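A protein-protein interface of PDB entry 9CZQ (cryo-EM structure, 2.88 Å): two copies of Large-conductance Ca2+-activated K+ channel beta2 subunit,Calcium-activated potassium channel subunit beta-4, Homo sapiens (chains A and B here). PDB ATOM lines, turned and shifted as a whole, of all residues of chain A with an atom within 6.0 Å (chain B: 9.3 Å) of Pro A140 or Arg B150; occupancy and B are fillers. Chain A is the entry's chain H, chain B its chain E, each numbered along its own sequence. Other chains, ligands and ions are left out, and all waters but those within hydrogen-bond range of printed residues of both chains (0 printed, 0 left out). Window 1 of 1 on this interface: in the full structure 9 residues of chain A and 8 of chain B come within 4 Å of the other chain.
Of the printed residues of chain A, Arg B150 touches Leu A128, His A130, Pro A140, Asp A186 and Asp A187.
Printed residues of chain B within 4 Å of His A130: Arg B150.
Of the printed residues of chain B, Lys A141 touches Phe B99 and Asn B152.
Of the printed residues of chain A, Cys B105 touches Leu A137 and Pro A140.
Of the printed residues of chain B, Asp A186 touches Arg B150.
Printed residues of chain B within 4 Å of Asp A187: Arg B150 (2.9 Å).
Thr B100 touches none of the printed residues of chain A.
The nearest residue of chain A that does not touch Arg B150 is Lys A141 (4.5 Å).
No position is printed for both chains.
SG of Cys B101 forms a disulfide with SG of Cys B105, 1.5 Å away.
The side-chain amide nitrogen (ND2) of Asn B152 lies within hydrogen-bond range of the side-chain amide oxygen (OE1) of Gln B110 (2.8 Å).
The backbone NH of Phe B99 is in hydrogen-bond range of the backbone carbonyl oxygen of Gly B107 (2.9 Å).
A ring nitrogen (ND1) of His A130 lies within hydrogen-bond range of the side-chain amide oxygen (OE1) of Gln A135 (2.8 Å).
OD1 of Asp B104 lies within salt-bridge range of NH2 of Arg B106, at 2.9 Å.
The backbone NH (N) of Lys A141 sits close to the side-chain amide oxygen (OD1) of Asn A139.
Arg B150 touches Leu A128.
NH1 of Arg B150 touches NE2 of His A130, 3.98 Å away.
CD2 of Leu A137 touches O of Asp B104, at 3.8 Å.
Leu A137 touches Cys B105.
Cys B101 touches Pro A140.
Cys B105 touches Pro A140.
Lys A141 touches Phe B99 (CB to CZ, 3.7 Å).
NZ of Lys A141 touches OD1 of Asn B152, at 3.8 Å.
Of the 13 printed residues of chain A, 7 touch a printed residue of chain B.
Hydrophobic or aromatic side chains of chain A within 4 Å of the printed part of chain B: Leu A128, His A130, Leu A137 and Pro A140.
Of the 25 printed residues of chain B, 6 touch a printed residue of chain A.
Hydrophobic or aromatic side chains of chain B within 4 Å of the printed part of chain A: Phe B99.
Among the printed residues, 11 pairs touch across the chains.
The guanidinium group (NH2) of Arg B150 lies within salt-bridge range of the side-chain carboxylate (OD1) of Asp A186 (3.6 Å).
The guanidinium group of Arg B150 is in salt-bridge range of the side-chain carboxylate of Asp A187 (2.9 Å).
NH1 of Arg B150 is in hydrogen-bond range of O of Pro A140 (2.7 Å).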
ATOM      1  N   GLN A 115     -24.884  12.858  18.535  1.00  0.00           N
ATOM      2  CA  GLN A 115     -24.043  11.689  18.733  1.00  0.00           C
ATOM      3  C   GLN A 115     -24.424  10.617  17.716  1.00  0.00           C
ATOM      4  O   GLN A 115     -25.589  10.471  17.345  1.00  0.00           O
ATOM      5  CB  GLN A 115     -24.131  11.180  20.170  1.00  0.00           C
ATOM      6  CG  GLN A 115     -23.447  12.135  21.160  1.00  0.00           C
ATOM      7  CD  GLN A 115     -23.313  11.531  22.556  1.00  0.00           C
ATOM      8  OE1 GLN A 115     -23.901  10.510  22.886  1.00  0.00           O
ATOM      9  NE2 GLN A 115     -22.527  12.115  23.433  1.00  0.00           N
ATOM     10  N   LEU A 128     -18.407   5.496  19.595  1.00  0.00           N
ATOM     11  CA  LEU A 128     -18.927   6.801  19.170  1.00  0.00           C
ATOM     12  C   LEU A 128     -18.123   7.323  17.979  1.00  0.00           C
ATOM     13  O   LEU A 128     -16.895   7.388  18.012  1.00  0.00           O
ATOM     14  CB  LEU A 128     -18.872   7.754  20.375  1.00  0.00           C
ATOM     15  CG  LEU A 128     -19.164   9.244  20.104  1.00  0.00           C
ATOM     16  CD1 LEU A 128     -20.503   9.513  19.428  1.00  0.00           C
ATOM     17  CD2 LEU A 128     -19.192   9.987  21.436  1.00  0.00           C
ATOM     18  N   HIS A 130     -16.616  10.095  15.435  1.00  0.00           N
ATOM     19  CA  HIS A 130     -16.023  11.404  15.460  1.00  0.00           C
ATOM     20  C   HIS A 130     -15.431  11.683  14.090  1.00  0.00           C
ATOM     21  O   HIS A 130     -14.635  10.957  13.657  1.00  0.00           O
ATOM     22  CB  HIS A 130     -14.957  11.436  16.518  1.00  0.00           C
ATOM     23  CG  HIS A 130     -15.440  11.519  17.915  1.00  0.00           C
ATOM     24  ND1 HIS A 130     -15.921  12.634  18.518  1.00  0.00           N
ATOM     25  CD2 HIS A 130     -15.535  10.514  18.815  1.00  0.00           C
ATOM     26  CE1 HIS A 130     -16.256  12.329  19.764  1.00  0.00           C
ATOM     27  NE2 HIS A 130     -16.030  11.042  20.002  1.00  0.00           N
ATOM     28  N   GLN A 135     -11.823  16.903  15.488  1.00  0.00           N
ATOM     29  CA  GLN A 135     -13.173  16.933  16.041  1.00  0.00           C
ATOM     30  C   GLN A 135     -13.239  16.173  17.371  1.00  0.00           C
ATOM     31  O   GLN A 135     -13.742  16.716  18.356  1.00  0.00           O
ATOM     32  CB  GLN A 135     -14.187  16.425  15.007  1.00  0.00           C
ATOM     33  CG  GLN A 135     -15.633  16.750  15.404  1.00  0.00           C
ATOM     34  CD  GLN A 135     -16.178  15.904  16.548  1.00  0.00           C
ATOM     35  OE1 GLN A 135     -15.930  14.718  16.653  1.00  0.00           O
ATOM     36  NE2 GLN A 135     -16.936  16.477  17.457  1.00  0.00           N
ATOM     37  N   LEU A 136     -12.662  14.968  17.439  1.00  0.00           N
ATOM     38  CA  LEU A 136     -12.555  14.200  18.680  1.00  0.00           C
ATOM     39  C   LEU A 136     -11.912  15.034  19.790  1.00  0.00           C
ATOM     40  O   LEU A 136     -12.406  15.046  20.905  1.00  0.00           O
ATOM     41  CB  LEU A 136     -11.761  12.906  18.425  1.00  0.00           C
ATOM     42  CG  LEU A 136     -11.315  12.141  19.683  1.00  0.00           C
ATOM     43  CD1 LEU A 136     -12.478  11.655  20.534  1.00  0.00           C
ATOM     44  CD2 LEU A 136     -10.500  10.915  19.281  1.00  0.00           C
ATOM     45  N   LEU A 137     -10.822  15.745  19.509  1.00  0.00           N
ATOM     46  CA  LEU A 137     -10.107  16.494  20.534  1.00  0.00           C
ATOM     47  C   LEU A 137     -10.725  17.866  20.844  1.00  0.00           C
ATOM     48  O   LEU A 137     -10.640  18.315  21.984  1.00  0.00           O
ATOM     49  CB  LEU A 137      -8.630  16.571  20.129  1.00  0.00           C
ATOM     50  CG  LEU A 137      -7.901  15.213  20.187  1.00  0.00           C
ATOM     51  CD1 LEU A 137      -6.494  15.359  19.615  1.00  0.00           C
ATOM     52  CD2 LEU A 137      -7.773  14.693  21.620  1.00  0.00           C
ATOM     53  N   THR A 138     -11.371  18.547  19.892  1.00  0.00           N
ATOM     54  CA  THR A 138     -12.034  19.839  20.154  1.00  0.00           C
ATOM     55  C   THR A 138     -13.346  19.686  20.933  1.00  0.00           C
ATOM     56  O   THR A 138     -13.687  20.557  21.730  1.00  0.00           O
ATOM     57  CB  THR A 138     -12.224  20.665  18.867  1.00  0.00           C
ATOM     58  OG1 THR A 138     -12.407  22.023  19.198  1.00  0.00           O
ATOM     59  CG2 THR A 138     -13.438  20.280  18.029  1.00  0.00           C
ATOM     60  N   ASN A 139     -14.065  18.566  20.765  1.00  0.00           N
ATOM     61  CA  ASN A 139     -15.251  18.237  21.558  1.00  0.00           C
ATOM     62  C   ASN A 139     -15.483  16.709  21.640  1.00  0.00           C
ATOM     63  O   ASN A 139     -16.337  16.170  20.937  1.00  0.00           O
ATOM     64  CB  ASN A 139     -16.472  18.988  20.998  1.00  0.00           C
ATOM     65  CG  ASN A 139     -17.672  18.882  21.924  1.00  0.00           C
ATOM     66  OD1 ASN A 139     -17.679  18.151  22.898  1.00  0.00           O
ATOM     67  ND2 ASN A 139     -18.713  19.630  21.668  1.00  0.00           N
ATOM     68  N   PRO A 140     -14.780  15.987  22.529  1.00  0.00           N
ATOM     69  CA  PRO A 140     -14.893  14.528  22.648  1.00  0.00           C
ATOM     70  C   PRO A 140     -16.257  14.051  23.148  1.00  0.00           C
ATOM     71  O   PRO A 140     -16.619  12.890  22.971  1.00  0.00           O
ATOM     72  CB  PRO A 140     -13.789  14.110  23.619  1.00  0.00           C
ATOM     73  CG  PRO A 140     -13.502  15.380  24.416  1.00  0.00           C
ATOM     74  CD  PRO A 140     -13.765  16.504  23.428  1.00  0.00           C
ATOM     75  N   LYS A 141     -17.036  14.944  23.754  1.00  0.00           N
ATOM     76  CA  LYS A 141     -18.418  14.732  24.197  1.00  0.00           C
ATOM     77  C   LYS A 141     -19.421  14.686  23.024  1.00  0.00           C
ATOM     78  O   LYS A 141     -20.560  14.267  23.229  1.00  0.00           O
ATOM     79  CB  LYS A 141     -18.667  15.840  25.244  1.00  0.00           C
ATOM     80  CG  LYS A 141     -20.089  16.249  25.614  1.00  0.00           C
ATOM     81  CD  LYS A 141     -20.854  15.307  26.553  1.00  0.00           C
ATOM     82  CE  LYS A 141     -22.103  16.108  26.949  1.00  0.00           C
ATOM     83  NZ  LYS A 141     -22.952  15.493  27.992  1.00  0.00           N
ATOM     84  N   CYS A 142     -19.026  15.052  21.799  1.00  0.00           N
ATOM     85  CA  CYS A 142     -19.937  15.221  20.660  1.00  0.00           C
ATOM     86  C   CYS A 142     -19.388  14.671  19.326  1.00  0.00           C
ATOM     87  O   CYS A 142     -18.178  14.582  19.151  1.00  0.00           O
ATOM     88  CB  CYS A 142     -20.265  16.713  20.562  1.00  0.00           C
ATOM     89  SG  CYS A 142     -21.777  17.006  19.644  1.00  0.00           S
ATOM     90  N   ASP A 186     -13.228   3.530  22.643  1.00  0.00           N
ATOM     91  CA  ASP A 186     -14.626   3.492  22.205  1.00  0.00           C
ATOM     92  C   ASP A 186     -14.976   4.701  21.309  1.00  0.00           C
ATOM     93  O   ASP A 186     -16.119   5.157  21.275  1.00  0.00           O
ATOM     94  CB  ASP A 186     -15.580   3.283  23.399  1.00  0.00           C
ATOM     95  CG  ASP A 186     -15.454   4.270  24.575  1.00  0.00           C
ATOM     96  OD1 ASP A 186     -14.699   5.262  24.503  1.00  0.00           O
ATOM     97  OD2 ASP A 186     -16.125   4.024  25.608  1.00  0.00           O
ATOM     98  N   ASP A 187     -13.991   5.187  20.540  1.00  0.00           N
ATOM     99  CA  ASP A 187     -14.106   6.316  19.606  1.00  0.00           C
ATOM    100  C   ASP A 187     -13.638   5.921  18.191  1.00  0.00           C
ATOM    101  O   ASP A 187     -12.641   5.223  18.040  1.00  0.00           O
ATOM    102  CB  ASP A 187     -13.321   7.544  20.101  1.00  0.00           C
ATOM    103  CG  ASP A 187     -13.918   8.262  21.318  1.00  0.00           C
ATOM    104  OD1 ASP A 187     -15.096   8.010  21.645  1.00  0.00           O
ATOM    105  OD2 ASP A 187     -13.185   9.034  21.971  1.00  0.00           O
ATOM    106  N   CYS B  97     -17.076  16.926  36.527  1.00  0.00           N
ATOM    107  CA  CYS B  97     -15.838  16.142  36.462  1.00  0.00           C
ATOM    108  C   CYS B  97     -15.223  16.270  35.068  1.00  0.00           C
ATOM    109  O   CYS B  97     -15.902  16.603  34.094  1.00  0.00           O
ATOM    110  CB  CYS B  97     -16.038  14.680  36.899  1.00  0.00           C
ATOM    111  SG  CYS B  97     -17.159  13.610  35.956  1.00  0.00           S
ATOM    112  N   THR B  98     -13.923  16.007  34.968  1.00  0.00           N
ATOM    113  CA  THR B  98     -13.190  15.993  33.696  1.00  0.00           C
ATOM    114  C   THR B  98     -12.972  14.551  33.252  1.00  0.00           C
ATOM    115  O   THR B  98     -12.490  13.737  34.036  1.00  0.00           O
ATOM    116  CB  THR B  98     -11.850  16.724  33.845  1.00  0.00           C
ATOM    117  OG1 THR B  98     -12.083  18.074  34.191  1.00  0.00           O
ATOM    118  CG2 THR B  98     -11.031  16.742  32.561  1.00  0.00           C
ATOM    119  N   PHE B  99     -13.299  14.229  32.002  1.00  0.00           N
ATOM    120  CA  PHE B  99     -13.069  12.913  31.400  1.00  0.00           C
ATOM    121  C   PHE B  99     -12.006  13.001  30.305  1.00  0.00           C
ATOM    122  O   PHE B  99     -11.877  14.017  29.625  1.00  0.00           O
ATOM    123  CB  PHE B  99     -14.374  12.302  30.877  1.00  0.00           C
ATOM    124  CG  PHE B  99     -14.956  12.958  29.643  1.00  0.00           C
ATOM    125  CD1 PHE B  99     -15.765  14.098  29.775  1.00  0.00           C
ATOM    126  CD2 PHE B  99     -14.725  12.411  28.367  1.00  0.00           C
ATOM    127  CE1 PHE B  99     -16.343  14.684  28.640  1.00  0.00           C
ATOM    128  CE2 PHE B  99     -15.317  12.988  27.234  1.00  0.00           C
ATOM    129  CZ  PHE B  99     -16.131  14.123  27.370  1.00  0.00           C
ATOM    130  N   THR B 100     -11.215  11.943  30.161  1.00  0.00           N
ATOM    131  CA  THR B 100      -9.945  11.949  29.422  1.00  0.00           C
ATOM    132  C   THR B 100      -9.948  10.939  28.275  1.00  0.00           C
ATOM    133  O   THR B 100     -10.635   9.924  28.320  1.00  0.00           O
ATOM    134  CB  THR B 100      -8.763  11.707  30.368  1.00  0.00           C
ATOM    135  OG1 THR B 100      -8.892  10.489  31.043  1.00  0.00           O
ATOM    136  CG2 THR B 100      -8.646  12.791  31.424  1.00  0.00           C
ATOM    137  N   CYS B 101      -9.166  11.253  27.229  1.00  0.00           N
ATOM    138  CA  CYS B 101      -9.083  10.425  26.011  1.00  0.00           C
ATOM    139  C   CYS B 101      -7.778  10.409  25.171  1.00  0.00           C
ATOM    140  O   CYS B 101      -7.847  10.591  23.956  1.00  0.00           O
ATOM    141  CB  CYS B 101     -10.238  10.790  25.056  1.00  0.00           C
ATOM    142  SG  CYS B 101     -10.380  12.541  24.591  1.00  0.00           S
ATOM    143  N   GLY B 102      -6.608  10.190  25.779  1.00  0.00           N
ATOM    144  CA  GLY B 102      -5.346  10.122  25.030  1.00  0.00           C
ATOM    145  C   GLY B 102      -4.686  11.435  24.613  1.00  0.00           C
ATOM    146  O   GLY B 102      -5.399  12.365  24.256  1.00  0.00           O
ATOM    147  N   ASP B 104      -3.628  14.885  24.647  1.00  0.00           N
ATOM    148  CA  ASP B 104      -4.346  15.757  25.578  1.00  0.00           C
ATOM    149  C   ASP B 104      -5.685  16.124  24.917  1.00  0.00           C
ATOM    150  O   ASP B 104      -5.736  16.883  23.948  1.00  0.00           O
ATOM    151  CB  ASP B 104      -3.456  16.955  25.939  1.00  0.00           C
ATOM    152  CG  ASP B 104      -4.016  17.820  27.071  1.00  0.00           C
ATOM    153  OD1 ASP B 104      -5.209  17.692  27.404  1.00  0.00           O
ATOM    154  OD2 ASP B 104      -3.256  18.642  27.628  1.00  0.00           O
ATOM    155  N   CYS B 105      -6.765  15.515  25.422  1.00  0.00           N
ATOM    156  CA  CYS B 105      -8.068  15.407  24.747  1.00  0.00           C
ATOM    157  C   CYS B 105      -9.282  15.906  25.557  1.00  0.00           C
ATOM    158  O   CYS B 105     -10.395  15.962  25.044  1.00  0.00           O
ATOM    159  CB  CYS B 105      -8.190  13.943  24.307  1.00  0.00           C
ATOM    160  SG  CYS B 105      -9.700  13.393  23.491  1.00  0.00           S
ATOM    161  N   ARG B 106      -9.099  16.202  26.846  1.00  0.00           N
ATOM    162  CA  ARG B 106     -10.169  16.205  27.858  1.00  0.00           C
ATOM    163  C   ARG B 106     -11.381  17.109  27.587  1.00  0.00           C
ATOM    164  O   ARG B 106     -11.257  18.181  26.991  1.00  0.00           O
ATOM    165  CB  ARG B 106      -9.558  16.447  29.252  1.00  0.00           C
ATOM    166  CG  ARG B 106      -8.907  17.814  29.536  1.00  0.00           C
ATOM    167  CD  ARG B 106      -8.236  17.957  30.906  1.00  0.00           C
ATOM    168  NE  ARG B 106      -7.680  19.306  31.117  1.00  0.00           N
ATOM    169  CZ  ARG B 106      -6.515  19.763  30.707  1.00  0.00           C
ATOM    170  NH1 ARG B 106      -6.102  20.935  31.095  1.00  0.00           N
ATOM    171  NH2 ARG B 106      -5.747  19.092  29.905  1.00  0.00           N
ATOM    172  N   GLY B 107     -12.531  16.709  28.121  1.00  0.00           N
ATOM    173  CA  GLY B 107     -13.756  17.515  28.231  1.00  0.00           C
ATOM    174  C   GLY B 107     -14.413  17.351  29.605  1.00  0.00           C
ATOM    175  O   GLY B 107     -13.887  16.623  30.446  1.00  0.00           O
ATOM    176  N   THR B 108     -15.558  17.992  29.857  1.00  0.00           N
ATOM    177  CA  THR B 108     -16.251  17.884  31.157  1.00  0.00           C
ATOM    178  C   THR B 108     -17.671  17.334  31.057  1.00  0.00           C
ATOM    179  O   THR B 108     -18.388  17.528  30.071  1.00  0.00           O
ATOM    180  CB  THR B 108     -16.231  19.184  31.977  1.00  0.00           C
ATOM    181  OG1 THR B 108     -17.015  20.191  31.392  1.00  0.00           O
ATOM    182  CG2 THR B 108     -14.824  19.740  32.173  1.00  0.00           C
ATOM    183  N   SER B 109     -18.072  16.630  32.111  1.00  0.00           N
ATOM    184  CA  SER B 109     -19.383  16.003  32.273  1.00  0.00           C
ATOM    185  C   SER B 109     -19.915  16.267  33.671  1.00  0.00           C
ATOM    186  O   SER B 109     -19.148  16.326  34.631  1.00  0.00           O
ATOM    187  CB  SER B 109     -19.294  14.499  32.030  1.00  0.00           C
ATOM    188  OG  SER B 109     -18.918  14.239  30.698  1.00  0.00           O
ATOM    189  N   GLN B 110     -21.225  16.428  33.805  1.00  0.00           N
ATOM    190  CA  GLN B 110     -21.838  16.677  35.102  1.00  0.00           C
ATOM    191  C   GLN B 110     -21.904  15.400  35.947  1.00  0.00           C
ATOM    192  O   GLN B 110     -22.010  14.291  35.418  1.00  0.00           O
ATOM    193  CB  GLN B 110     -23.229  17.317  34.952  1.00  0.00           C
ATOM    194  CG  GLN B 110     -23.167  18.776  34.472  1.00  0.00           C
ATOM    195  CD  GLN B 110     -22.792  18.944  33.002  1.00  0.00           C
ATOM    196  OE1 GLN B 110     -23.204  18.192  32.132  1.00  0.00           O
ATOM    197  NE2 GLN B 110     -22.003  19.931  32.655  1.00  0.00           N
ATOM    198  N   TYR B 111     -21.911  15.558  37.266  1.00  0.00           N
ATOM    199  CA  TYR B 111     -22.357  14.546  38.220  1.00  0.00           C
ATOM    200  C   TYR B 111     -23.283  15.175  39.277  1.00  0.00           C
ATOM    201  O   TYR B 111     -23.087  16.335  39.651  1.00  0.00           O
ATOM    202  CB  TYR B 111     -21.158  13.816  38.838  1.00  0.00           C
ATOM    203  CG  TYR B 111     -20.208  14.667  39.658  1.00  0.00           C
ATOM    204  CD1 TYR B 111     -19.136  15.317  39.026  1.00  0.00           C
ATOM    205  CD2 TYR B 111     -20.366  14.768  41.052  1.00  0.00           C
ATOM    206  CE1 TYR B 111     -18.228  16.077  39.782  1.00  0.00           C
ATOM    207  CE2 TYR B 111     -19.462  15.535  41.812  1.00  0.00           C
ATOM    208  CZ  TYR B 111     -18.393  16.196  41.174  1.00  0.00           C
ATOM    209  OH  TYR B 111     -17.517  16.945  41.888  1.00  0.00           O
ATOM    210  N   PRO B 146     -17.751  10.518  41.242  1.00  0.00           N
ATOM    211  CA  PRO B 146     -17.528   9.359  40.392  1.00  0.00           C
ATOM    212  C   PRO B 146     -16.276   9.572  39.530  1.00  0.00           C
ATOM    213  O   PRO B 146     -16.060  10.681  39.040  1.00  0.00           O
ATOM    214  CB  PRO B 146     -18.791   9.245  39.538  1.00  0.00           C
ATOM    215  CG  PRO B 146     -19.255  10.695  39.403  1.00  0.00           C
ATOM    216  CD  PRO B 146     -18.855  11.320  40.737  1.00  0.00           C
ATOM    217  N   PRO B 147     -15.465   8.538  39.264  1.00  0.00           N
ATOM    218  CA  PRO B 147     -14.529   8.563  38.147  1.00  0.00           C
ATOM    219  C   PRO B 147     -15.309   8.840  36.856  1.00  0.00           C
ATOM    220  O   PRO B 147     -16.241   8.103  36.552  1.00  0.00           O
ATOM    221  CB  PRO B 147     -13.869   7.185  38.136  1.00  0.00           C
ATOM    222  CG  PRO B 147     -14.148   6.626  39.501  1.00  0.00           C
ATOM    223  CD  PRO B 147     -15.461   7.245  39.907  1.00  0.00           C
ATOM    224  N   CYS B 148     -14.976   9.958  36.225  1.00  0.00           N
ATOM    225  CA  CYS B 148     -15.624  10.432  35.016  1.00  0.00           C
ATOM    226  C   CYS B 148     -15.491   9.458  33.854  1.00  0.00           C
ATOM    227  O   CYS B 148     -14.401   9.256  33.318  1.00  0.00           O
ATOM    228  CB  CYS B 148     -15.046  11.798  34.643  1.00  0.00           C
ATOM    229  SG  CYS B 148     -15.377  13.128  35.820  1.00  0.00           S
ATOM    230  N   LYS B 149     -16.637   8.894  33.478  1.00  0.00           N
ATOM    231  CA  LYS B 149     -16.741   7.929  32.396  1.00  0.00           C
ATOM    232  C   LYS B 149     -17.659   8.403  31.269  1.00  0.00           C
ATOM    233  O   LYS B 149     -18.778   7.910  31.117  1.00  0.00           O
ATOM    234  CB  LYS B 149     -17.229   6.583  32.933  1.00  0.00           C
ATOM    235  CG  LYS B 149     -16.262   5.909  33.891  1.00  0.00           C
ATOM    236  CD  LYS B 149     -16.812   4.580  34.381  1.00  0.00           C
ATOM    237  CE  LYS B 149     -15.869   3.928  35.378  1.00  0.00           C
ATOM    238  NZ  LYS B 149     -14.554   3.595  34.761  1.00  0.00           N
ATOM    239  N   ARG B 150     -17.161   9.384  30.518  1.00  0.00           N
ATOM    240  CA  ARG B 150     -17.836  10.003  29.370  1.00  0.00           C
ATOM    241  C   ARG B 150     -19.149  10.753  29.640  1.00  0.00           C
ATOM    242  O   ARG B 150     -19.133  11.908  30.063  1.00  0.00           O
ATOM    243  CB  ARG B 150     -17.999   9.014  28.205  1.00  0.00           C
ATOM    244  CG  ARG B 150     -16.684   8.502  27.637  1.00  0.00           C
ATOM    245  CD  ARG B 150     -15.871   9.626  27.016  1.00  0.00           C
ATOM    246  NE  ARG B 150     -16.581  10.261  25.910  1.00  0.00           N
ATOM    247  CZ  ARG B 150     -16.612   9.780  24.671  1.00  0.00           C
ATOM    248  NH1 ARG B 150     -17.284  10.423  23.726  1.00  0.00           N
ATOM    249  NH2 ARG B 150     -15.970   8.659  24.374  1.00  0.00           N
ATOM    250  N   GLU B 151     -20.275  10.093  29.391  1.00  0.00           N
ATOM    251  CA  GLU B 151     -21.591  10.720  29.532  1.00  0.00           C
ATOM    252  C   GLU B 151     -22.206  10.835  30.931  1.00  0.00           C
ATOM    253  O   GLU B 151     -22.032   9.972  31.790  1.00  0.00           O
ATOM    254  CB  GLU B 151     -22.595  10.044  28.591  1.00  0.00           C
ATOM    255  CG  GLU B 151     -22.765   8.554  28.833  1.00  0.00           C
ATOM    256  CD  GLU B 151     -21.892   7.713  27.923  1.00  0.00           C
ATOM    257  OE1 GLU B 151     -21.546   8.190  26.822  1.00  0.00           O
ATOM    258  OE2 GLU B 151     -21.552   6.576  28.309  1.00  0.00           O
ATOM    259  N   ASN B 152     -22.938  11.931  31.116  1.00  0.00           N
ATOM    260  CA  ASN B 152     -23.665  12.259  32.348  1.00  0.00           C
ATOM    261  C   ASN B 152     -24.481  11.093  32.922  1.00  0.00           C
ATOM    262  O   ASN B 152     -24.528  10.909  34.137  1.00  0.00           O
ATOM    263  CB  ASN B 152     -24.600  13.444  32.072  1.00  0.00           C
ATOM    264  CG  ASN B 152     -23.903  14.767  31.828  1.00  0.00           C
ATOM    265  OD1 ASN B 152     -22.687  14.879  31.773  1.00  0.00           O
ATOM    266  ND2 ASN B 152     -24.660  15.824  31.687  1.00  0.00           N
ATOM    267  N   GLN B 153     -25.087  10.271  32.061  1.00  0.00           N
ATOM    268  CA  GLN B 153     -25.918   9.145  32.488  1.00  0.00           C
ATOM    269  C   GLN B 153     -25.123   8.137  33.322  1.00  0.00           C
ATOM    270  O   GLN B 153     -25.614   7.655  34.338  1.00  0.00           O
ATOM    271  CB  GLN B 153     -26.541   8.450  31.262  1.00  0.00           C
ATOM    272  CG  GLN B 153     -27.300   9.395  30.318  1.00  0.00           C
ATOM    273  CD  GLN B 153     -28.263  10.320  31.055  1.00  0.00           C
ATOM    274  OE1 GLN B 153     -28.027  11.509  31.201  1.00  0.00           O
ATOM    275  NE2 GLN B 153     -29.354   9.815  31.581  1.00  0.00           N
ATOM    276  N   LYS B 154     -23.875   7.856  32.936  1.00  0.00           N
ATOM    277  CA  LYS B 154     -23.003   6.906  33.638  1.00  0.00           C
ATOM    278  C   LYS B 154     -22.483   7.474  34.959  1.00  0.00           C
ATOM    279  O   LYS B 154     -22.351   6.739  35.932  1.00  0.00           O
ATOM    280  CB  LYS B 154     -21.838   6.498  32.727  1.00  0.00           C
ATOM    281  CG  LYS B 154     -22.248   5.859  31.395  1.00  0.00           C
ATOM    282  CD  LYS B 154     -23.071   4.581  31.563  1.00  0.00           C
ATOM    283  CE  LYS B 154     -23.178   3.794  30.255  1.00  0.00           C
ATOM    284  NZ  LYS B 154     -23.908   4.520  29.193  1.00  0.00           N
ATOM    285  N   ASN B 155     -22.250   8.785  35.029  1.00  0.00           N
ATOM    286  CA  ASN B 155     -21.925   9.453  36.290  1.00  0.00           C
ATOM    287  C   ASN B 155     -23.101   9.382  37.272  1.00  0.00           C
ATOM    288  O   ASN B 155     -22.917   8.978  38.417  1.00  0.00           O
ATOM    289  CB  ASN B 155     -21.527  10.910  36.033  1.00  0.00           C
ATOM    290  CG  ASN B 155     -20.219  11.092  35.302  1.00  0.00           C
ATOM    291  OD1 ASN B 155     -19.413  10.191  35.163  1.00  0.00           O
ATOM    292  ND2 ASN B 155     -19.967  12.286  34.835  1.00  0.00           N
ATOM    293  N   LEU B 156     -24.315   9.723  36.830  1.00  0.00           N
ATOM    294  CA  LEU B 156     -25.510   9.649  37.669  1.00  0.00           C
ATOM    295  C   LEU B 156     -25.805   8.211  38.106  1.00  0.00           C
ATOM    296  O   LEU B 156     -26.052   7.978  39.282  1.00  0.00           O
ATOM    297  CB  LEU B 156     -26.685  10.304  36.926  1.00  0.00           C
ATOM    298  CG  LEU B 156     -27.992  10.309  37.744  1.00  0.00           C
ATOM    299  CD1 LEU B 156     -28.761  11.605  37.513  1.00  0.00           C
ATOM    300  CD2 LEU B 156     -28.918   9.157  37.358  1.00  0.00           C
